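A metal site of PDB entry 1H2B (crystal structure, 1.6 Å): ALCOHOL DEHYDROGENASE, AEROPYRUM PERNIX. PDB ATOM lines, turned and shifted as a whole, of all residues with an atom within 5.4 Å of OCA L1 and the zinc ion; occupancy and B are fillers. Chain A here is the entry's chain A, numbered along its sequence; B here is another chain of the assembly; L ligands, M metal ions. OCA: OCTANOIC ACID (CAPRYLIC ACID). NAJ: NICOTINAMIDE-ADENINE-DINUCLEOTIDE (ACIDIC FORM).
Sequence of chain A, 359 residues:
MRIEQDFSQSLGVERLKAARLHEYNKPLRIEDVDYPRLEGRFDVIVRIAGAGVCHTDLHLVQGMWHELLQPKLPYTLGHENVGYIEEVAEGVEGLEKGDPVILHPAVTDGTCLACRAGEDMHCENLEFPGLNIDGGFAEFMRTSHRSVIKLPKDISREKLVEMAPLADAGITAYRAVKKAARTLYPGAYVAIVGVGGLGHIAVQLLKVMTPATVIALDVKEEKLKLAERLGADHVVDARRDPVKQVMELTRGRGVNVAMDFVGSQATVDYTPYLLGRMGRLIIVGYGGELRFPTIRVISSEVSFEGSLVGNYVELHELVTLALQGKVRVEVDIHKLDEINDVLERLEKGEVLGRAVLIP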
ATOM      1  N   CYS A  54       5.298  -2.737  -8.353  1.00  0.00           N
ATOM      2  CA  CYS A  54       5.506  -3.894  -7.508  1.00  0.00           C
ATOM      3  C   CYS A  54       6.320  -4.967  -8.240  1.00  0.00           C
ATOM      4  O   CYS A  54       6.269  -5.046  -9.461  1.00  0.00           O
ATOM      5  CB  CYS A  54       4.124  -4.469  -7.145  1.00  0.00           C
ATOM      6  SG  CYS A  54       4.111  -5.883  -6.029  1.00  0.00           S
ATOM      7  N   THR A  56       5.436  -7.833  -8.463  1.00  0.00           N
ATOM      8  CA  THR A  56       4.378  -8.587  -9.156  1.00  0.00           C
ATOM      9  C   THR A  56       4.226  -8.110 -10.586  1.00  0.00           C
ATOM     10  O   THR A  56       3.856  -8.917 -11.465  1.00  0.00           O
ATOM     11  CB  THR A  56       3.065  -8.454  -8.372  1.00  0.00           C
ATOM     12  OG1 THR A  56       3.152  -9.308  -7.227  1.00  0.00           O
ATOM     13  CG2 THR A  56       1.840  -8.945  -9.184  1.00  0.00           C
ATOM     14  N   TRP A  65       1.253 -15.082 -14.341  1.00  0.00           N
ATOM     15  CA  TRP A  65      -0.143 -15.111 -13.927  1.00  0.00           C
ATOM     16  C   TRP A  65      -1.109 -15.497 -15.062  1.00  0.00           C
ATOM     17  O   TRP A  65      -2.325 -15.538 -14.847  1.00  0.00           O
ATOM     18  CB  TRP A  65      -0.560 -13.752 -13.372  1.00  0.00           C
ATOM     19  CG  TRP A  65      -0.001 -13.528 -11.997  1.00  0.00           C
ATOM     20  CD1 TRP A  65       1.123 -12.781 -11.663  1.00  0.00           C
ATOM     21  CD2 TRP A  65      -0.511 -14.037 -10.780  1.00  0.00           C
ATOM     22  NE1 TRP A  65       1.314 -12.795 -10.300  1.00  0.00           N
ATOM     23  CE2 TRP A  65       0.336 -13.571  -9.727  1.00  0.00           C
ATOM     24  CE3 TRP A  65      -1.615 -14.844 -10.435  1.00  0.00           C
ATOM     25  CZ2 TRP A  65       0.107 -13.874  -8.384  1.00  0.00           C
ATOM     26  CZ3 TRP A  65      -1.827 -15.141  -9.083  1.00  0.00           C
ATOM     27  CH2 TRP A  65      -0.963 -14.663  -8.091  1.00  0.00           C
ATOM     28  N   HIS A  79      -1.367  -1.681  -9.333  1.00  0.00           N
ATOM     29  CA  HIS A  79      -2.368  -2.093  -8.304  1.00  0.00           C
ATOM     30  C   HIS A  79      -2.095  -1.483  -6.916  1.00  0.00           C
ATOM     31  O   HIS A  79      -2.629  -1.966  -5.887  1.00  0.00           O
ATOM     32  CB  HIS A  79      -2.439  -3.631  -8.218  1.00  0.00           C
ATOM     33  CG  HIS A  79      -1.120  -4.304  -7.968  1.00  0.00           C
ATOM     34  ND1 HIS A  79      -0.240  -4.621  -8.980  1.00  0.00           N
ATOM     35  CD2 HIS A  79      -0.536  -4.717  -6.814  1.00  0.00           C
ATOM     36  CE1 HIS A  79       0.835  -5.190  -8.462  1.00  0.00           C
ATOM     37  NE2 HIS A  79       0.687  -5.280  -7.147  1.00  0.00           N
ATOM     38  N   GLU A  80      -1.282  -0.430  -6.915  1.00  0.00           N
ATOM     39  CA  GLU A  80      -0.839   0.212  -5.664  1.00  0.00           C
ATOM     40  C   GLU A  80      -1.078   1.707  -5.716  1.00  0.00           C
ATOM     41  O   GLU A  80      -0.165   2.524  -5.972  1.00  0.00           O
ATOM     42  CB  GLU A  80       0.654  -0.080  -5.490  1.00  0.00           C
ATOM     43  CG  GLU A  80       1.190   0.205  -4.083  1.00  0.00           C
ATOM     44  CD  GLU A  80       2.553  -0.449  -3.905  1.00  0.00           C
ATOM     45  OE1 GLU A  80       3.553   0.207  -4.255  1.00  0.00           O
ATOM     46  OE2 GLU A  80       2.641  -1.599  -3.409  1.00  0.00           O
ATOM     47  N   MET A 121      -9.846 -10.689   0.317  1.00  0.00           N
ATOM     48  CA  MET A 121      -9.093 -11.378  -0.735  1.00  0.00           C
ATOM     49  C   MET A 121      -9.650 -12.727  -1.028  1.00  0.00           C
ATOM     50  O   MET A 121      -9.180 -13.417  -1.944  1.00  0.00           O
ATOM     51  CB  MET A 121      -7.600 -11.519  -0.337  1.00  0.00           C
ATOM     52  CG  MET A 121      -6.907 -10.174  -0.120  1.00  0.00           C
ATOM     53  SD  MET A 121      -6.959  -9.147  -1.582  1.00  0.00           S
ATOM     54  CE  MET A 121      -6.196 -10.250  -2.862  1.00  0.00           C
ATOM     55  N   LEU A 126     -14.018 -11.708  -6.910  1.00  0.00           N
ATOM     56  CA  LEU A 126     -12.915 -10.738  -6.837  1.00  0.00           C
ATOM     57  C   LEU A 126     -12.442 -10.247  -8.216  1.00  0.00           C
ATOM     58  O   LEU A 126     -12.163 -11.059  -9.122  1.00  0.00           O
ATOM     59  CB  LEU A 126     -11.742 -11.359  -6.055  1.00  0.00           C
ATOM     60  CG  LEU A 126     -10.721 -10.290  -5.642  1.00  0.00           C
ATOM     61  CD1 LEU A 126     -10.397 -10.420  -4.180  1.00  0.00           C
ATOM     62  CD2 LEU A 126      -9.464 -10.374  -6.503  1.00  0.00           C
ATOM     63  N   PHE A 128      -9.301  -7.322  -9.600  1.00  0.00           N
ATOM     64  CA  PHE A 128      -8.099  -6.746  -9.033  1.00  0.00           C
ATOM     65  C   PHE A 128      -7.472  -5.794 -10.056  1.00  0.00           C
ATOM     66  O   PHE A 128      -6.704  -6.246 -10.916  1.00  0.00           O
ATOM     67  CB  PHE A 128      -7.188  -7.926  -8.681  1.00  0.00           C
ATOM     68  CG  PHE A 128      -6.144  -7.632  -7.616  1.00  0.00           C
ATOM     69  CD1 PHE A 128      -6.274  -8.131  -6.328  1.00  0.00           C
ATOM     70  CD2 PHE A 128      -5.005  -6.885  -7.905  1.00  0.00           C
ATOM     71  CE1 PHE A 128      -5.292  -7.880  -5.322  1.00  0.00           C
ATOM     72  CE2 PHE A 128      -4.015  -6.649  -6.927  1.00  0.00           C
ATOM     73  CZ  PHE A 128      -4.154  -7.150  -5.642  1.00  0.00           C
ATOM     74  N   LEU A 131      -4.080  -6.287 -12.100  1.00  0.00           N
ATOM     75  CA  LEU A 131      -3.699  -7.704 -12.161  1.00  0.00           C
ATOM     76  C   LEU A 131      -4.421  -8.428 -13.259  1.00  0.00           C
ATOM     77  O   LEU A 131      -3.764  -9.036 -14.089  1.00  0.00           O
ATOM     78  CB  LEU A 131      -3.895  -8.452 -10.829  1.00  0.00           C
ATOM     79  CG  LEU A 131      -2.463  -8.749 -10.340  1.00  0.00           C
ATOM     80  CD1 LEU A 131      -1.922  -7.681  -9.399  1.00  0.00           C
ATOM     81  CD2 LEU A 131      -2.253 -10.139  -9.808  1.00  0.00           C
ATOM     82  N   ASP A 168      -0.504  -1.859  -1.256  1.00  0.00           N
ATOM     83  CA  ASP A 168      -0.221  -3.232  -1.618  1.00  0.00           C
ATOM     84  C   ASP A 168       1.016  -3.735  -0.892  1.00  0.00           C
ATOM     85  O   ASP A 168       0.945  -4.686  -0.120  1.00  0.00           O
ATOM     86  CB  ASP A 168      -0.092  -3.341  -3.160  1.00  0.00           C
ATOM     87  CG  ASP A 168       0.113  -4.744  -3.600  1.00  0.00           C
ATOM     88  OD1 ASP A 168       1.215  -5.053  -4.068  1.00  0.00           O
ATOM     89  OD2 ASP A 168      -0.754  -5.633  -3.460  1.00  0.00           O
ATOM     90  N   THR A 172       0.280  -5.858   2.545  1.00  0.00           N
ATOM     91  CA  THR A 172       0.754  -7.255   2.497  1.00  0.00           C
ATOM     92  C   THR A 172       1.760  -7.522   3.615  1.00  0.00           C
ATOM     93  O   THR A 172       1.650  -8.524   4.333  1.00  0.00           O
ATOM     94  CB  THR A 172       1.404  -7.554   1.160  1.00  0.00           C
ATOM     95  OG1 THR A 172       0.444  -7.337   0.139  1.00  0.00           O
ATOM     96  CG2 THR A 172       1.804  -9.019   1.070  1.00  0.00           C
ATOM     97  N   TYR A 286       6.670 -14.859  -4.176  1.00  0.00           N
ATOM     98  CA  TYR A 286       6.396 -16.114  -4.877  1.00  0.00           C
ATOM     99  C   TYR A 286       7.169 -16.142  -6.177  1.00  0.00           C
ATOM    100  O   TYR A 286       7.737 -15.168  -6.619  1.00  0.00           O
ATOM    101  CB  TYR A 286       4.881 -16.262  -5.115  1.00  0.00           C
ATOM    102  CG  TYR A 286       4.340 -15.123  -5.942  1.00  0.00           C
ATOM    103  CD1 TYR A 286       4.312 -15.176  -7.331  1.00  0.00           C
ATOM    104  CD2 TYR A 286       3.875 -13.956  -5.321  1.00  0.00           C
ATOM    105  CE1 TYR A 286       3.841 -14.097  -8.079  1.00  0.00           C
ATOM    106  CE2 TYR A 286       3.407 -12.861  -6.062  1.00  0.00           C
ATOM    107  CZ  TYR A 286       3.412 -12.948  -7.451  1.00  0.00           C
ATOM    108  OH  TYR A 286       3.013 -11.895  -8.188  1.00  0.00           O
ATOM    109  N   LEU A 308      -1.602 -13.362   1.870  1.00  0.00           N
ATOM    110  CA  LEU A 308      -2.082 -12.773   0.643  1.00  0.00           C
ATOM    111  C   LEU A 308      -2.632 -11.371   0.874  1.00  0.00           C
ATOM    112  O   LEU A 308      -3.698 -11.202   1.505  1.00  0.00           O
ATOM    113  CB  LEU A 308      -3.160 -13.696   0.037  1.00  0.00           C
ATOM    114  CG  LEU A 308      -3.889 -13.151  -1.205  1.00  0.00           C
ATOM    115  CD1 LEU A 308      -2.925 -13.030  -2.399  1.00  0.00           C
ATOM    116  CD2 LEU A 308      -5.093 -14.041  -1.573  1.00  0.00           C
ATOM    117  N   VAL A 309      -1.911 -10.370   0.351  1.00  0.00           N
ATOM    118  CA  VAL A 309      -2.348  -8.974   0.439  1.00  0.00           C
ATOM    119  C   VAL A 309      -2.901  -8.720   1.839  1.00  0.00           C
ATOM    120  O   VAL A 309      -2.200  -8.973   2.819  1.00  0.00           O
ATOM    121  CB  VAL A 309      -3.253  -8.536  -0.764  1.00  0.00           C
ATOM    122  CG1 VAL A 309      -3.336  -7.007  -0.885  1.00  0.00           C
ATOM    123  CG2 VAL A 309      -2.692  -9.103  -2.116  1.00  0.00           C
ATOM    124  N   ARG A 354      10.648   1.461  -2.551  1.00  0.00           N
ATOM    125  CA  ARG A 354       9.539   1.349  -3.505  1.00  0.00           C
ATOM    126  C   ARG A 354       9.524   2.467  -4.514  1.00  0.00           C
ATOM    127  O   ARG A 354       9.494   3.609  -4.148  1.00  0.00           O
ATOM    128  CB  ARG A 354       8.206   1.382  -2.737  1.00  0.00           C
ATOM    129  CG  ARG A 354       6.966   0.920  -3.494  1.00  0.00           C
ATOM    130  CD  ARG A 354       7.111  -0.407  -4.172  1.00  0.00           C
ATOM    131  NE  ARG A 354       5.923  -1.217  -4.109  1.00  0.00           N
ATOM    132  CZ  ARG A 354       5.976  -2.540  -4.220  1.00  0.00           C
ATOM    133  NH1 ARG A 354       7.148  -3.170  -4.356  1.00  0.00           N
ATOM    134  NH2 ARG A 354       4.818  -3.214  -4.179  1.00  0.00           N
ATOM    135  N   ARG B 277      -9.561 -22.237  -0.331  1.00  0.00           N
ATOM    136  CA  ARG B 277      -8.971 -20.938   0.037  1.00  0.00           C
ATOM    137  C   ARG B 277      -8.832 -20.895   1.532  1.00  0.00           C
ATOM    138  O   ARG B 277      -9.760 -21.266   2.313  1.00  0.00           O
ATOM    139  CB  ARG B 277      -9.835 -19.785  -0.453  1.00  0.00           C
ATOM    140  CG  ARG B 277      -9.902 -19.715  -1.971  1.00  0.00           C
ATOM    141  CD  ARG B 277     -10.527 -18.414  -2.531  1.00  0.00           C
ATOM    142  NE  ARG B 277      -9.599 -17.288  -2.436  1.00  0.00           N
ATOM    143  CZ  ARG B 277      -8.520 -17.099  -3.203  1.00  0.00           C
ATOM    144  NH1 ARG B 277      -8.190 -17.923  -4.199  1.00  0.00           N
ATOM    145  NH2 ARG B 277      -7.759 -16.023  -2.985  1.00  0.00           N
ATOM    146  N   ILE B 298       0.495 -18.533  -2.024  1.00  0.00           N
ATOM    147  CA  ILE B 298      -0.033 -17.191  -1.734  1.00  0.00           C
ATOM    148  C   ILE B 298      -1.405 -16.966  -2.383  1.00  0.00           C
ATOM    149  O   ILE B 298      -2.279 -16.350  -1.746  1.00  0.00           O
ATOM    150  CB  ILE B 298       1.020 -16.064  -2.028  1.00  0.00           C
ATOM    151  CG1 ILE B 298       1.209 -15.830  -3.522  1.00  0.00           C
ATOM    152  CG2 ILE B 298       2.345 -16.386  -1.348  1.00  0.00           C
ATOM    153  CD1 ILE B 298       0.299 -14.777  -4.136  1.00  0.00           C
ATOM    154  N   SER B 299      -1.643 -17.443  -3.605  1.00  0.00           N
ATOM    155  CA  SER B 299      -2.920 -17.068  -4.252  1.00  0.00           C
ATOM    156  C   SER B 299      -4.123 -17.721  -3.568  1.00  0.00           C
ATOM    157  O   SER B 299      -5.202 -17.126  -3.588  1.00  0.00           O
ATOM    158  CB  SER B 299      -2.913 -17.298  -5.763  1.00  0.00           C
ATOM    159  OG  SER B 299      -2.707 -18.657  -5.988  1.00  0.00           O
HETATM  160  C1  OCA L   1       0.140  -8.430  -5.450  1.00  0.00           C
HETATM  161  C2  OCA L   1      -0.187  -9.887  -5.740  1.00  0.00           C
HETATM  162  C3  OCA L   1      -1.690 -10.139  -5.573  1.00  0.00           C
HETATM  163  C4  OCA L   1      -2.176 -11.377  -6.323  1.00  0.00           C
HETATM  164  C5  OCA L   1      -3.652 -11.594  -5.984  1.00  0.00           C
HETATM  165  C6  OCA L   1      -4.051 -13.059  -6.135  1.00  0.00           C
HETATM  166  C7  OCA L   1      -5.583 -13.184  -6.028  1.00  0.00           C
HETATM  167  C8  OCA L   1      -6.042 -14.545  -5.509  1.00  0.00           C
HETATM  168  O1  OCA L   1       1.277  -7.972  -5.815  1.00  0.00           O
HETATM  169  O2  OCA L   1      -0.741  -7.695  -4.930  1.00  0.00           O
HETATM  170  PA  NAJ L   2      11.421  -6.169  -4.530  1.00  0.00           P
HETATM  171  O1A NAJ L   2      12.050  -6.488  -5.884  1.00  0.00           O
HETATM  172  O2A NAJ L   2      11.249  -4.703  -4.165  1.00  0.00           O
HETATM  173  O5B NAJ L   2      12.263  -6.763  -3.342  1.00  0.00           O
HETATM  174  C5B NAJ L   2      12.883  -8.047  -3.374  1.00  0.00           C
HETATM  175  C4B NAJ L   2      14.036  -7.958  -2.379  1.00  0.00           C
HETATM  176  O4B NAJ L   2      14.625  -9.236  -2.291  1.00  0.00           O
HETATM  177  C3B NAJ L   2      15.186  -7.010  -2.844  1.00  0.00           C
HETATM  178  O3B NAJ L   2      15.504  -6.075  -1.829  1.00  0.00           O
HETATM  179  C2B NAJ L   2      16.273  -7.983  -3.243  1.00  0.00           C
HETATM  180  O2B NAJ L   2      17.601  -7.470  -3.229  1.00  0.00           O
HETATM  181  C1B NAJ L   2      16.046  -9.099  -2.243  1.00  0.00           C
HETATM  182  N9A NAJ L   2      16.651 -10.358  -2.655  1.00  0.00           N
HETATM  183  C8A NAJ L   2      16.836 -10.893  -3.913  1.00  0.00           C
HETATM  184  N7A NAJ L   2      17.400 -12.108  -3.769  1.00  0.00           N
HETATM  185  C5A NAJ L   2      17.582 -12.362  -2.432  1.00  0.00           C
HETATM  186  C6A NAJ L   2      18.143 -13.412  -1.716  1.00  0.00           C
HETATM  187  N6A NAJ L   2      18.652 -14.505  -2.305  1.00  0.00           N
HETATM  188  N1A NAJ L   2      18.163 -13.370  -0.327  1.00  0.00           N
HETATM  189  C2A NAJ L   2      17.684 -12.219   0.306  1.00  0.00           C
HETATM  190  N3A NAJ L   2      17.157 -11.186  -0.378  1.00  0.00           N
HETATM  191  C4A NAJ L   2      17.105 -11.248  -1.739  1.00  0.00           C
HETATM  192  O3  NAJ L   2      10.030  -6.961  -4.535  1.00  0.00           O
HETATM  193  PN  NAJ L   2       8.653  -6.571  -3.796  1.00  0.00           P
HETATM  194  O1N NAJ L   2       7.875  -5.697  -4.689  1.00  0.00           O
HETATM  195  O2N NAJ L   2       8.975  -6.216  -2.401  1.00  0.00           O
HETATM  196  O5D NAJ L   2       7.957  -8.008  -3.823  1.00  0.00           O
HETATM  197  C5D NAJ L   2       8.504  -9.056  -3.038  1.00  0.00           C
HETATM  198  C4D NAJ L   2       7.861 -10.413  -3.386  1.00  0.00           C
HETATM  199  O4D NAJ L   2       6.494 -10.383  -2.903  1.00  0.00           O
HETATM  200  C3D NAJ L   2       7.693 -10.637  -4.901  1.00  0.00           C
HETATM  201  O3D NAJ L   2       7.790 -12.020  -5.149  1.00  0.00           O
HETATM  202  C2D NAJ L   2       6.310 -10.110  -5.213  1.00  0.00           C
HETATM  203  O2D NAJ L   2       5.756 -10.600  -6.407  1.00  0.00           O
HETATM  204  C1D NAJ L   2       5.597 -10.645  -3.976  1.00  0.00           C
HETATM  205  N1N NAJ L   2       4.276 -10.071  -3.663  1.00  0.00           N
HETATM  206  C2N NAJ L   2       3.470 -10.866  -2.896  1.00  0.00           C
HETATM  207  C3N NAJ L   2       2.257 -10.370  -2.456  1.00  0.00           C
HETATM  208  C7N NAJ L   2       1.353 -11.296  -1.676  1.00  0.00           C
HETATM  209  O7N NAJ L   2       0.167 -10.795  -1.377  1.00  0.00           O
HETATM  210  N7N NAJ L   2       1.715 -12.518  -1.324  1.00  0.00           N
HETATM  211  C4N NAJ L   2       1.842  -9.029  -2.708  1.00  0.00           C
HETATM  212  C5N NAJ L   2       2.781  -8.181  -3.357  1.00  0.00           C
HETATM  213  C6N NAJ L   2       3.983  -8.721  -3.796  1.00  0.00           C
HETATM  214 ZN    ZN M   1       1.889  -6.129  -5.766  1.00  0.00          ZN
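The side-chain hydroxyl of Thr 56 sits close to an oxygen (O1) of OCA L1 (2.7 Å).
An oxygen (O2D) of NAJ L2 lies within hydrogen-bond range of the backbone NH of Thr 56 (3.5 Å).
The side-chain hydroxyl (OG1) of Thr 56 is in hydrogen-bond range of an oxygen (O2D) of NAJ L2, at 3.0 Å.
O7N of NAJ L2 is in hydrogen-bond range of N of Val 309 (2.7 Å).
An oxygen (O1N) of NAJ L2 is in salt-bridge range of the guanidinium group of Arg 354 (2.7 Å).
An oxygen (O3D) of NAJ L2 sits at hydrogen-bond distance from the backbone NH of Tyr 286.
An oxygen (O3D) of NAJ L2 lies within hydrogen-bond range of the backbone carbonyl oxygen (O) of Tyr 286, 3.5 Å away.
O of Asp 168 lies within hydrogen-bond range of OG1 of Thr 172 (2.7 Å).
SG of Cys 54 sits close to N of Thr 56, at 3.4 Å.
The side-chain sulfur of Cys 54 lies close to the guanidinium group of Arg 354 (3.3 Å).
The side-chain hydroxyl of Thr 56 lies within hydrogen-bond range of the side-chain hydroxyl of Tyr 286, 2.8 Å away.
NH2 of Arg 277 of chain B is in hydrogen-bond range of O of Ser 299 of chain B, 2.8 Å away.
The guanidinium group (NH2) of Arg 277 of chain B lies within hydrogen-bond range of the backbone carbonyl oxygen (O) of Met 121 (3.1 Å).
The indole nitrogen (NE1) of Trp 65 is in hydrogen-bond range of the side-chain hydroxyl (OH) of Tyr 286 (2.9 Å).
Trp 65 touches OCA L1 (CH2 to C4, 3.9 Å).
Phe 128 touches OCA L1 (CZ to O2, 3.5 Å).
Leu 131 touches OCA L1 (CD2 to C4, 3.7 Å).
CD1 of Leu 308 touches C6 of OCA L1 (3.9 Å).
Val 309 touches OCA L1 (CG2 to O2, 3.7 Å).
Arg 277 of chain B touches OCA L1 (NH2 to C8, 3.4 Å).
O of Ser 299 of chain B touches C8 of OCA L1, at 3.3 Å.
Hydrophobic or aromatic side chains that line OCA L1: Trp 65, His 79, Phe 128, Leu 131, Leu 308 and Val 309.
11 residues have an atom within 4 Å of OCA L1: Cys 54, Thr 56, Trp 65, His 79, Phe 128, Leu 131, Asp 168, Leu 308, Val 309, Arg 277 of chain B and Ser 299 of chain B.
The zinc ion is bound by an oxygen (O1) of OCA L1 (1.9 Å), a ring nitrogen (NE2) of His 79 (2.0 Å), the side-chain carboxylate of Asp 168 (2.1 Å) and the side-chain sulfur of Cys 54 (2.3 Å).
Merely in contact with the zinc ion: Thr 56 (3.7 Å).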
